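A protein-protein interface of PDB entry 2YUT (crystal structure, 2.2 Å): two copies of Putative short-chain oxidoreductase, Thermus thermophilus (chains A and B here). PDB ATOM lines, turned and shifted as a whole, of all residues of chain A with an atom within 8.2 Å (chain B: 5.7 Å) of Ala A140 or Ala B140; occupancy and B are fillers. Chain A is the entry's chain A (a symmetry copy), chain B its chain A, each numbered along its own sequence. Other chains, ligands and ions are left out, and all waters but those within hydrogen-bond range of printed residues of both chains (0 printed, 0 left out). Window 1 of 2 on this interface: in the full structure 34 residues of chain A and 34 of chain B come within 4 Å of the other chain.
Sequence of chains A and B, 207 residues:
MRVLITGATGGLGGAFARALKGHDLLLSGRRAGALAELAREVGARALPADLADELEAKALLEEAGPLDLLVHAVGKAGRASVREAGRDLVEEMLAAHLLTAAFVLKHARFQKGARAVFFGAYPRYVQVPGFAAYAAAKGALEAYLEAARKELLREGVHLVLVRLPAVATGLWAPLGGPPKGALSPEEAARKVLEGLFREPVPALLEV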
ATOM      1  N   VAL A  90      14.956 -13.164  -9.528  1.00  0.00           N
ATOM      2  CA  VAL A  90      13.743 -13.466  -8.777  1.00  0.00           C
ATOM      3  C   VAL A  90      12.830 -14.417  -9.553  1.00  0.00           C
ATOM      4  O   VAL A  90      12.342 -15.404  -9.006  1.00  0.00           O
ATOM      5  CB  VAL A  90      12.958 -12.179  -8.425  1.00  0.00           C
ATOM      6  CG1 VAL A  90      11.658 -12.533  -7.708  1.00  0.00           C
ATOM      7  CG2 VAL A  90      13.809 -11.289  -7.534  1.00  0.00           C
ATOM      8  N   MET A  93      14.419 -17.927  -9.811  1.00  0.00           N
ATOM      9  CA  MET A  93      14.352 -18.617  -8.529  1.00  0.00           C
ATOM     10  C   MET A  93      12.960 -19.180  -8.267  1.00  0.00           C
ATOM     11  O   MET A  93      12.819 -20.330  -7.845  1.00  0.00           O
ATOM     12  CB  MET A  93      14.753 -17.671  -7.397  1.00  0.00           C
ATOM     13  CG  MET A  93      16.246 -17.362  -7.337  1.00  0.00           C
ATOM     14  SD  MET A  93      17.357 -18.952  -7.061  1.00  0.00           S
ATOM     15  CE  MET A  93      17.972 -19.177  -8.885  1.00  0.00           C
ATOM     16  N   LEU A  94      11.936 -18.367  -8.514  1.00  0.00           N
ATOM     17  CA  LEU A  94      10.556 -18.800  -8.315  1.00  0.00           C
ATOM     18  C   LEU A  94      10.201 -19.940  -9.268  1.00  0.00           C
ATOM     19  O   LEU A  94       9.498 -20.876  -8.896  1.00  0.00           O
ATOM     20  CB  LEU A  94       9.589 -17.626  -8.521  1.00  0.00           C
ATOM     21  CG  LEU A  94       9.354 -16.692  -7.322  1.00  0.00           C
ATOM     22  CD1 LEU A  94       8.639 -17.460  -6.226  1.00  0.00           C
ATOM     23  CD2 LEU A  94      10.672 -16.150  -6.792  1.00  0.00           C
ATOM     24  N   HIS A  97      12.287 -23.197  -7.997  1.00  0.00           N
ATOM     25  CA  HIS A  97      11.808 -23.739  -6.722  1.00  0.00           C
ATOM     26  C   HIS A  97      10.306 -23.944  -6.558  1.00  0.00           C
ATOM     27  O   HIS A  97       9.875 -24.991  -6.070  1.00  0.00           O
ATOM     28  CB  HIS A  97      12.277 -22.870  -5.552  1.00  0.00           C
ATOM     29  CG  HIS A  97      13.761 -22.800  -5.400  1.00  0.00           C
ATOM     30  ND1 HIS A  97      14.546 -21.943  -6.140  1.00  0.00           N
ATOM     31  CD2 HIS A  97      14.603 -23.460  -4.568  1.00  0.00           C
ATOM     32  CE1 HIS A  97      15.808 -22.073  -5.767  1.00  0.00           C
ATOM     33  NE2 HIS A  97      15.868 -22.986  -4.814  1.00  0.00           N
ATOM     34  N   LEU A  98       9.516 -22.950  -6.954  1.00  0.00           N
ATOM     35  CA  LEU A  98       8.067 -23.009  -6.780  1.00  0.00           C
ATOM     36  C   LEU A  98       7.244 -23.578  -7.928  1.00  0.00           C
ATOM     37  O   LEU A  98       6.404 -24.455  -7.711  1.00  0.00           O
ATOM     38  CB  LEU A  98       7.532 -21.611  -6.428  1.00  0.00           C
ATOM     39  CG  LEU A  98       6.019 -21.467  -6.229  1.00  0.00           C
ATOM     40  CD1 LEU A  98       5.588 -22.273  -5.010  1.00  0.00           C
ATOM     41  CD2 LEU A  98       5.655 -19.994  -6.048  1.00  0.00           C
ATOM     42  N   LEU A  99       7.459 -23.078  -9.139  1.00  0.00           N
ATOM     43  CA  LEU A  99       6.690 -23.558 -10.275  1.00  0.00           C
ATOM     44  C   LEU A  99       6.932 -25.044 -10.535  1.00  0.00           C
ATOM     45  O   LEU A  99       5.992 -25.775 -10.840  1.00  0.00           O
ATOM     46  CB  LEU A  99       7.001 -22.728 -11.524  1.00  0.00           C
ATOM     47  CG  LEU A  99       6.645 -21.235 -11.430  1.00  0.00           C
ATOM     48  CD1 LEU A  99       6.790 -20.604 -12.804  1.00  0.00           C
ATOM     49  CD2 LEU A  99       5.217 -21.048 -10.926  1.00  0.00           C
ATOM     50  N   GLN A 127      17.348 -15.723   4.709  1.00  0.00           N
ATOM     51  CA  GLN A 127      16.836 -14.357   4.680  1.00  0.00           C
ATOM     52  C   GLN A 127      17.909 -13.367   5.108  1.00  0.00           C
ATOM     53  O   GLN A 127      17.818 -12.742   6.164  1.00  0.00           O
ATOM     54  CB  GLN A 127      15.600 -14.251   5.571  1.00  0.00           C
ATOM     55  CG  GLN A 127      14.361 -14.828   4.896  1.00  0.00           C
ATOM     56  CD  GLN A 127      13.233 -15.104   5.867  1.00  0.00           C
ATOM     57  OE1 GLN A 127      13.163 -14.505   6.937  1.00  0.00           O
ATOM     58  NE2 GLN A 127      12.334 -16.006   5.486  1.00  0.00           N
ATOM     59  N   ALA A 132      17.967 -12.604  -1.279  1.00  0.00           N
ATOM     60  CA  ALA A 132      16.546 -12.261  -1.277  1.00  0.00           C
ATOM     61  C   ALA A 132      15.742 -13.123  -2.250  1.00  0.00           C
ATOM     62  O   ALA A 132      14.706 -13.679  -1.887  1.00  0.00           O
ATOM     63  CB  ALA A 132      16.365 -10.790  -1.620  1.00  0.00           C
ATOM     64  N   ALA A 133      16.219 -13.234  -3.483  1.00  0.00           N
ATOM     65  CA  ALA A 133      15.524 -14.029  -4.487  1.00  0.00           C
ATOM     66  C   ALA A 133      15.351 -15.481  -4.018  1.00  0.00           C
ATOM     67  O   ALA A 133      14.242 -16.013  -4.028  1.00  0.00           O
ATOM     68  CB  ALA A 133      16.282 -13.975  -5.808  1.00  0.00           C
ATOM     69  N   TYR A 134      16.446 -16.110  -3.594  1.00  0.00           N
ATOM     70  CA  TYR A 134      16.413 -17.493  -3.116  1.00  0.00           C
ATOM     71  C   TYR A 134      15.482 -17.614  -1.914  1.00  0.00           C
ATOM     72  O   TYR A 134      14.659 -18.529  -1.838  1.00  0.00           O
ATOM     73  CB  TYR A 134      17.820 -17.953  -2.701  1.00  0.00           C
ATOM     74  CG  TYR A 134      17.902 -19.418  -2.297  1.00  0.00           C
ATOM     75  CD1 TYR A 134      18.107 -20.414  -3.253  1.00  0.00           C
ATOM     76  CD2 TYR A 134      17.771 -19.804  -0.963  1.00  0.00           C
ATOM     77  CE1 TYR A 134      18.185 -21.761  -2.891  1.00  0.00           C
ATOM     78  CE2 TYR A 134      17.849 -21.157  -0.587  1.00  0.00           C
ATOM     79  CZ  TYR A 134      18.056 -22.125  -1.562  1.00  0.00           C
ATOM     80  OH  TYR A 134      18.145 -23.453  -1.214  1.00  0.00           O
ATOM     81  N   ALA A 135      15.628 -16.691  -0.967  1.00  0.00           N
ATOM     82  CA  ALA A 135      14.802 -16.691   0.237  1.00  0.00           C
ATOM     83  C   ALA A 135      13.322 -16.608  -0.123  1.00  0.00           C
ATOM     84  O   ALA A 135      12.496 -17.320   0.444  1.00  0.00           O
ATOM     85  CB  ALA A 135      15.188 -15.520   1.137  1.00  0.00           C
ATOM     86  N   ALA A 136      12.997 -15.727  -1.066  1.00  0.00           N
ATOM     87  CA  ALA A 136      11.621 -15.540  -1.503  1.00  0.00           C
ATOM     88  C   ALA A 136      11.053 -16.833  -2.088  1.00  0.00           C
ATOM     89  O   ALA A 136       9.933 -17.232  -1.765  1.00  0.00           O
ATOM     90  CB  ALA A 136      11.550 -14.427  -2.548  1.00  0.00           C
ATOM     91  N   ALA A 137      11.826 -17.473  -2.959  1.00  0.00           N
ATOM     92  CA  ALA A 137      11.386 -18.713  -3.587  1.00  0.00           C
ATOM     93  C   ALA A 137      11.070 -19.783  -2.546  1.00  0.00           C
ATOM     94  O   ALA A 137      10.068 -20.486  -2.664  1.00  0.00           O
ATOM     95  CB  ALA A 137      12.448 -19.213  -4.557  1.00  0.00           C
ATOM     96  N   LYS A 138      11.924 -19.904  -1.528  1.00  0.00           N
ATOM     97  CA  LYS A 138      11.705 -20.897  -0.472  1.00  0.00           C
ATOM     98  C   LYS A 138      10.572 -20.475   0.449  1.00  0.00           C
ATOM     99  O   LYS A 138       9.830 -21.317   0.958  1.00  0.00           O
ATOM    100  CB  LYS A 138      12.980 -21.116   0.351  1.00  0.00           C
ATOM    101  CG  LYS A 138      14.081 -21.861  -0.396  1.00  0.00           C
ATOM    102  CD  LYS A 138      13.600 -23.216  -0.907  1.00  0.00           C
ATOM    103  CE  LYS A 138      14.767 -24.060  -1.429  1.00  0.00           C
ATOM    104  NZ  LYS A 138      14.286 -25.266  -2.178  1.00  0.00           N
ATOM    105  N   GLY A 139      10.444 -19.167   0.671  1.00  0.00           N
ATOM    106  CA  GLY A 139       9.372 -18.687   1.517  1.00  0.00           C
ATOM    107  C   GLY A 139       8.046 -19.022   0.854  1.00  0.00           C
ATOM    108  O   GLY A 139       7.086 -19.406   1.518  1.00  0.00           O
ATOM    109  N   ALA A 140       8.004 -18.887  -0.467  1.00  0.00           N
ATOM    110  CA  ALA A 140       6.797 -19.174  -1.239  1.00  0.00           C
ATOM    111  C   ALA A 140       6.488 -20.670  -1.242  1.00  0.00           C
ATOM    112  O   ALA A 140       5.338 -21.077  -1.069  1.00  0.00           O
ATOM    113  CB  ALA A 140       6.966 -18.679  -2.671  1.00  0.00           C
ATOM    114  N   LEU A 141       7.521 -21.484  -1.437  1.00  0.00           N
ATOM    115  CA  LEU A 141       7.345 -22.925  -1.474  1.00  0.00           C
ATOM    116  C   LEU A 141       6.764 -23.455  -0.174  1.00  0.00           C
ATOM    117  O   LEU A 141       5.831 -24.251  -0.192  1.00  0.00           O
ATOM    118  CB  LEU A 141       8.678 -23.630  -1.758  1.00  0.00           C
ATOM    119  CG  LEU A 141       8.622 -25.166  -1.756  1.00  0.00           C
ATOM    120  CD1 LEU A 141       7.589 -25.642  -2.775  1.00  0.00           C
ATOM    121  CD2 LEU A 141       9.992 -25.746  -2.082  1.00  0.00           C
ATOM    122  N   GLU A 142       7.309 -23.011   0.955  1.00  0.00           N
ATOM    123  CA  GLU A 142       6.831 -23.478   2.251  1.00  0.00           C
ATOM    124  C   GLU A 142       5.396 -23.040   2.516  1.00  0.00           C
ATOM    125  O   GLU A 142       4.607 -23.799   3.076  1.00  0.00           O
ATOM    126  CB  GLU A 142       7.738 -22.979   3.385  1.00  0.00           C
ATOM    127  CG  GLU A 142       9.208 -23.357   3.239  1.00  0.00           C
ATOM    128  CD  GLU A 142       9.993 -23.158   4.531  1.00  0.00           C
ATOM    129  OE1 GLU A 142       9.684 -22.205   5.275  1.00  0.00           O
ATOM    130  OE2 GLU A 142      10.922 -23.945   4.802  1.00  0.00           O
ATOM    131  N   ALA A 143       5.058 -21.820   2.108  1.00  0.00           N
ATOM    132  CA  ALA A 143       3.710 -21.308   2.314  1.00  0.00           C
ATOM    133  C   ALA A 143       2.742 -22.085   1.435  1.00  0.00           C
ATOM    134  O   ALA A 143       1.648 -22.442   1.864  1.00  0.00           O
ATOM    135  CB  ALA A 143       3.649 -19.803   1.978  1.00  0.00           C
ATOM    136  N   TYR A 144       3.156 -22.349   0.201  1.00  0.00           N
ATOM    137  CA  TYR A 144       2.320 -23.084  -0.741  1.00  0.00           C
ATOM    138  C   TYR A 144       1.966 -24.470  -0.193  1.00  0.00           C
ATOM    139  O   TYR A 144       0.805 -24.890  -0.218  1.00  0.00           O
ATOM    140  CB  TYR A 144       3.061 -23.247  -2.066  1.00  0.00           C
ATOM    141  CG  TYR A 144       2.189 -23.738  -3.198  1.00  0.00           C
ATOM    142  CD1 TYR A 144       1.246 -22.896  -3.789  1.00  0.00           C
ATOM    143  CD2 TYR A 144       2.324 -25.032  -3.697  1.00  0.00           C
ATOM    144  CE1 TYR A 144       0.460 -23.328  -4.850  1.00  0.00           C
ATOM    145  CE2 TYR A 144       1.542 -25.476  -4.762  1.00  0.00           C
ATOM    146  CZ  TYR A 144       0.614 -24.617  -5.332  1.00  0.00           C
ATOM    147  OH  TYR A 144      -0.158 -25.044  -6.382  1.00  0.00           O
ATOM    148  N   LEU A 145       2.978 -25.166   0.314  1.00  0.00           N
ATOM    149  CA  LEU A 145       2.802 -26.511   0.847  1.00  0.00           C
ATOM    150  C   LEU A 145       1.950 -26.563   2.108  1.00  0.00           C
ATOM    151  O   LEU A 145       1.133 -27.466   2.270  1.00  0.00           O
ATOM    152  CB  LEU A 145       4.171 -27.146   1.120  1.00  0.00           C
ATOM    153  CG  LEU A 145       5.029 -27.365  -0.131  1.00  0.00           C
ATOM    154  CD1 LEU A 145       6.410 -27.871   0.265  1.00  0.00           C
ATOM    155  CD2 LEU A 145       4.342 -28.359  -1.057  1.00  0.00           C
ATOM    156  N   GLU A 146       2.138 -25.599   3.004  1.00  0.00           N
ATOM    157  CA  GLU A 146       1.363 -25.579   4.234  1.00  0.00           C
ATOM    158  C   GLU A 146      -0.114 -25.438   3.899  1.00  0.00           C
ATOM    159  O   GLU A 146      -0.962 -26.075   4.519  1.00  0.00           O
ATOM    160  CB  GLU A 146       1.814 -24.428   5.135  1.00  0.00           C
ATOM    161  CG  GLU A 146       1.019 -24.307   6.429  1.00  0.00           C
ATOM    162  CD  GLU A 146       0.875 -25.633   7.155  1.00  0.00           C
ATOM    163  OE1 GLU A 146       1.893 -26.339   7.315  1.00  0.00           O
ATOM    164  OE2 GLU A 146      -0.256 -25.966   7.571  1.00  0.00           O
ATOM    165  N   ALA A 147      -0.408 -24.616   2.896  1.00  0.00           N
ATOM    166  CA  ALA A 147      -1.783 -24.384   2.471  1.00  0.00           C
ATOM    167  C   ALA A 147      -2.369 -25.623   1.806  1.00  0.00           C
ATOM    168  O   ALA A 147      -3.533 -25.960   2.016  1.00  0.00           O
ATOM    169  CB  ALA A 147      -1.836 -23.203   1.499  1.00  0.00           C
ATOM    170  N   LEU B  94       2.195 -14.426  -7.909  1.00  0.00           N
ATOM    171  CA  LEU B  94       3.584 -14.032  -7.701  1.00  0.00           C
ATOM    172  C   LEU B  94       3.897 -12.734  -8.445  1.00  0.00           C
ATOM    173  O   LEU B  94       4.622 -11.879  -7.942  1.00  0.00           O
ATOM    174  CB  LEU B  94       4.535 -15.144  -8.167  1.00  0.00           C
ATOM    175  CG  LEU B  94       4.823 -16.280  -7.172  1.00  0.00           C
ATOM    176  CD1 LEU B  94       5.595 -15.723  -5.990  1.00  0.00           C
ATOM    177  CD2 LEU B  94       3.531 -16.917  -6.687  1.00  0.00           C
ATOM    178  N   LEU B  98       4.709 -10.197  -5.655  1.00  0.00           N
ATOM    179  CA  LEU B  98       6.164 -10.164  -5.544  1.00  0.00           C
ATOM    180  C   LEU B  98       6.933  -9.391  -6.606  1.00  0.00           C
ATOM    181  O   LEU B  98       7.786  -8.565  -6.274  1.00  0.00           O
ATOM    182  CB  LEU B  98       6.709 -11.601  -5.481  1.00  0.00           C
ATOM    183  CG  LEU B  98       8.230 -11.772  -5.386  1.00  0.00           C
ATOM    184  CD1 LEU B  98       8.724 -11.202  -4.062  1.00  0.00           C
ATOM    185  CD2 LEU B  98       8.595 -13.251  -5.496  1.00  0.00           C
ATOM    186  N   ALA B 135      -1.132 -17.476  -0.626  1.00  0.00           N
ATOM    187  CA  ALA B 135      -0.247 -17.693   0.516  1.00  0.00           C
ATOM    188  C   ALA B 135       1.213 -17.703   0.075  1.00  0.00           C
ATOM    189  O   ALA B 135       2.069 -17.102   0.721  1.00  0.00           O
ATOM    190  CB  ALA B 135      -0.594 -19.011   1.203  1.00  0.00           C
ATOM    191  N   ALA B 136       1.487 -18.393  -1.028  1.00  0.00           N
ATOM    192  CA  ALA B 136       2.840 -18.490  -1.560  1.00  0.00           C
ATOM    193  C   ALA B 136       3.384 -17.111  -1.924  1.00  0.00           C
ATOM    194  O   ALA B 136       4.520 -16.772  -1.589  1.00  0.00           O
ATOM    195  CB  ALA B 136       2.855 -19.393  -2.793  1.00  0.00           C
ATOM    196  N   ALA B 137       2.572 -16.324  -2.624  1.00  0.00           N
ATOM    197  CA  ALA B 137       2.986 -14.989  -3.035  1.00  0.00           C
ATOM    198  C   ALA B 137       3.358 -14.127  -1.832  1.00  0.00           C
ATOM    199  O   ALA B 137       4.357 -13.409  -1.867  1.00  0.00           O
ATOM    200  CB  ALA B 137       1.880 -14.324  -3.843  1.00  0.00           C
ATOM    201  N   LYS B 138       2.556 -14.198  -0.769  1.00  0.00           N
ATOM    202  CA  LYS B 138       2.830 -13.415   0.440  1.00  0.00           C
ATOM    203  C   LYS B 138       4.005 -13.994   1.212  1.00  0.00           C
ATOM    204  O   LYS B 138       4.775 -13.256   1.828  1.00  0.00           O
ATOM    205  CB  LYS B 138       1.597 -13.356   1.350  1.00  0.00           C
ATOM    206  CG  LYS B 138       0.464 -12.492   0.807  1.00  0.00           C
ATOM    207  CD  LYS B 138       0.926 -11.064   0.532  1.00  0.00           C
ATOM    208  CE  LYS B 138      -0.260 -10.144   0.231  1.00  0.00           C
ATOM    209  NZ  LYS B 138       0.188  -8.819  -0.307  1.00  0.00           N
ATOM    210  N   GLY B 139       4.137 -15.319   1.183  1.00  0.00           N
ATOM    211  CA  GLY B 139       5.247 -15.942   1.872  1.00  0.00           C
ATOM    212  C   GLY B 139       6.540 -15.485   1.219  1.00  0.00           C
ATOM    213  O   GLY B 139       7.534 -15.225   1.894  1.00  0.00           O
ATOM    214  N   ALA B 140       6.517 -15.375  -0.105  1.00  0.00           N
ATOM    215  CA  ALA B 140       7.686 -14.944  -0.870  1.00  0.00           C
ATOM    216  C   ALA B 140       8.002 -13.472  -0.613  1.00  0.00           C
ATOM    217  O   ALA B 140       9.160 -13.099  -0.424  1.00  0.00           O
ATOM    218  CB  ALA B 140       7.445 -15.169  -2.358  1.00  0.00           C
ATOM    219  N   LEU B 141       6.965 -12.642  -0.604  1.00  0.00           N
ATOM    220  CA  LEU B 141       7.145 -11.217  -0.385  1.00  0.00           C
ATOM    221  C   LEU B 141       7.791 -10.932   0.961  1.00  0.00           C
ATOM    222  O   LEU B 141       8.726 -10.143   1.042  1.00  0.00           O
ATOM    223  CB  LEU B 141       5.802 -10.478  -0.469  1.00  0.00           C
ATOM    224  CG  LEU B 141       5.865  -8.969  -0.189  1.00  0.00           C
ATOM    225  CD1 LEU B 141       6.850  -8.309  -1.152  1.00  0.00           C
ATOM    226  CD2 LEU B 141       4.483  -8.345  -0.335  1.00  0.00           C
ATOM    227  N   GLU B 142       7.300 -11.579   2.014  1.00  0.00           N
ATOM    228  CA  GLU B 142       7.844 -11.355   3.348  1.00  0.00           C
ATOM    229  C   GLU B 142       9.287 -11.827   3.458  1.00  0.00           C
ATOM    230  O   GLU B 142      10.106 -11.181   4.108  1.00  0.00           O
ATOM    231  CB  GLU B 142       6.991 -12.058   4.414  1.00  0.00           C
ATOM    232  CG  GLU B 142       5.516 -11.666   4.413  1.00  0.00           C
ATOM    233  CD  GLU B 142       4.795 -12.103   5.683  1.00  0.00           C
ATOM    234  OE1 GLU B 142       5.135 -13.174   6.223  1.00  0.00           O
ATOM    235  OE2 GLU B 142       3.883 -11.382   6.139  1.00  0.00           O
ATOM    236  N   ALA B 143       9.599 -12.951   2.818  1.00  0.00           N
ATOM    237  CA  ALA B 143      10.953 -13.486   2.859  1.00  0.00           C
ATOM    238  C   ALA B 143      11.881 -12.556   2.092  1.00  0.00           C
ATOM    239  O   ALA B 143      12.996 -12.278   2.525  1.00  0.00           O
ATOM    240  CB  ALA B 143      10.991 -14.903   2.251  1.00  0.00           C
ATOM    241  N   TYR B 144      11.408 -12.072   0.948  1.00  0.00           N
ATOM    242  CA  TYR B 144      12.200 -11.173   0.118  1.00  0.00           C
ATOM    243  C   TYR B 144      12.587  -9.910   0.894  1.00  0.00           C
ATOM    244  O   TYR B 144      13.748  -9.487   0.888  1.00  0.00           O
ATOM    245  CB  TYR B 144      11.397 -10.772  -1.117  1.00  0.00           C
ATOM    246  CG  TYR B 144      12.213 -10.079  -2.181  1.00  0.00           C
ATOM    247  CD1 TYR B 144      13.124 -10.794  -2.962  1.00  0.00           C
ATOM    248  CD2 TYR B 144      12.061  -8.715  -2.426  1.00  0.00           C
ATOM    249  CE1 TYR B 144      13.858 -10.171  -3.962  1.00  0.00           C
ATOM    250  CE2 TYR B 144      12.792  -8.080  -3.428  1.00  0.00           C
ATOM    251  CZ  TYR B 144      13.687  -8.816  -4.192  1.00  0.00           C
ATOM    252  OH  TYR B 144      14.408  -8.199  -5.182  1.00  0.00           O
ATOM    253  N   LEU B 145      11.604  -9.323   1.567  1.00  0.00           N
ATOM    254  CA  LEU B 145      11.812  -8.097   2.330  1.00  0.00           C
ATOM    255  C   LEU B 145      12.725  -8.274   3.535  1.00  0.00           C
ATOM    256  O   LEU B 145      13.553  -7.412   3.820  1.00  0.00           O
ATOM    257  CB  LEU B 145      10.461  -7.530   2.781  1.00  0.00           C
ATOM    258  CG  LEU B 145       9.544  -7.089   1.634  1.00  0.00           C
ATOM    259  CD1 LEU B 145       8.186  -6.670   2.183  1.00  0.00           C
ATOM    260  CD2 LEU B 145      10.189  -5.938   0.875  1.00  0.00           C
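The backbone carbonyl oxygen (O) of Leu A94 lies within hydrogen-bond range of the backbone NH (N) of Leu A99 (3.0 Å).
Among the printed residues, pairs that only touch across the chains: Ala A140 with Ala B136 (3.3 Å), Ala A136 with Ala B140 (3.3 Å), Ala A143 with Ala B135 (3.4 Å), Ala A135 with Ala B143 (3.4 Å), Ala A132 with Tyr B144 (3.5 Å), Leu A94 with Leu B94 (3.5 Å), Ala A140 with Ala B140 (3.6 Å), Gln A127 with Ala B143 (3.7 Å), Val A90 with Tyr B144 (3.7 Å), Leu A98 with Leu B94 (3.8 Å), Leu A94 with Leu B98 (3.8 Å), Val A90 with Leu B98 (3.8 Å), Ala A136 with Ala B143 (3.9 Å), Ala A143 with Ala B136 (3.9 Å), Gly A139 with Gly B139 (3.9 Å), Ala A133 with Tyr B144 (3.9 Å), Tyr A144 with Ala B136 (3.9 Å) and Ala A136 with Tyr B144 (3.9 Å).
Of the printed residues of chain B, Ala A140 touches Ala B136 and Ala B140. Of the printed residues of chain A, Gly B139 touches Gly A139 (3.9 Å). Printed residues of chain A within 4 Å of Ala B136: Ala A140, Ala A143 and Tyr A144. Of the printed residues of chain B, Ala A133 touches Tyr B144 (3.9 Å). Printed residues of chain B within 4 Å of Tyr A144: Ala B136. The nearest residue of chain A that does not touch Ala B140 is Gly A139 (4.1 Å). The nearest printed residue of chain B that does not touch Tyr A144 is Ala B135 (5.0 Å).
Hydrophobic or aromatic side chains of chain B within 4 Å of the printed part of chain A: Leu B94, Leu B98, Ala B136, Ala B140, Ala B143 and Tyr B144. Among the printed residues, 18 pairs touch across the chains. Among the printed residues, no Asp or Glu carboxylate lies within 4 Å of a Lys or Arg side-chain nitrogen of the other chain.
Ala A135 touches Ala B143, and with the chains exchanged Ala A143 touches Ala B135. Ala A136 touches Ala B140, and with the chains exchanged Ala A140 touches Ala B136. Ala A136 touches Ala B143, and with the chains exchanged Ala A143 touches Ala B136. Gly B139 touches its own counterpart, Gly A139.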
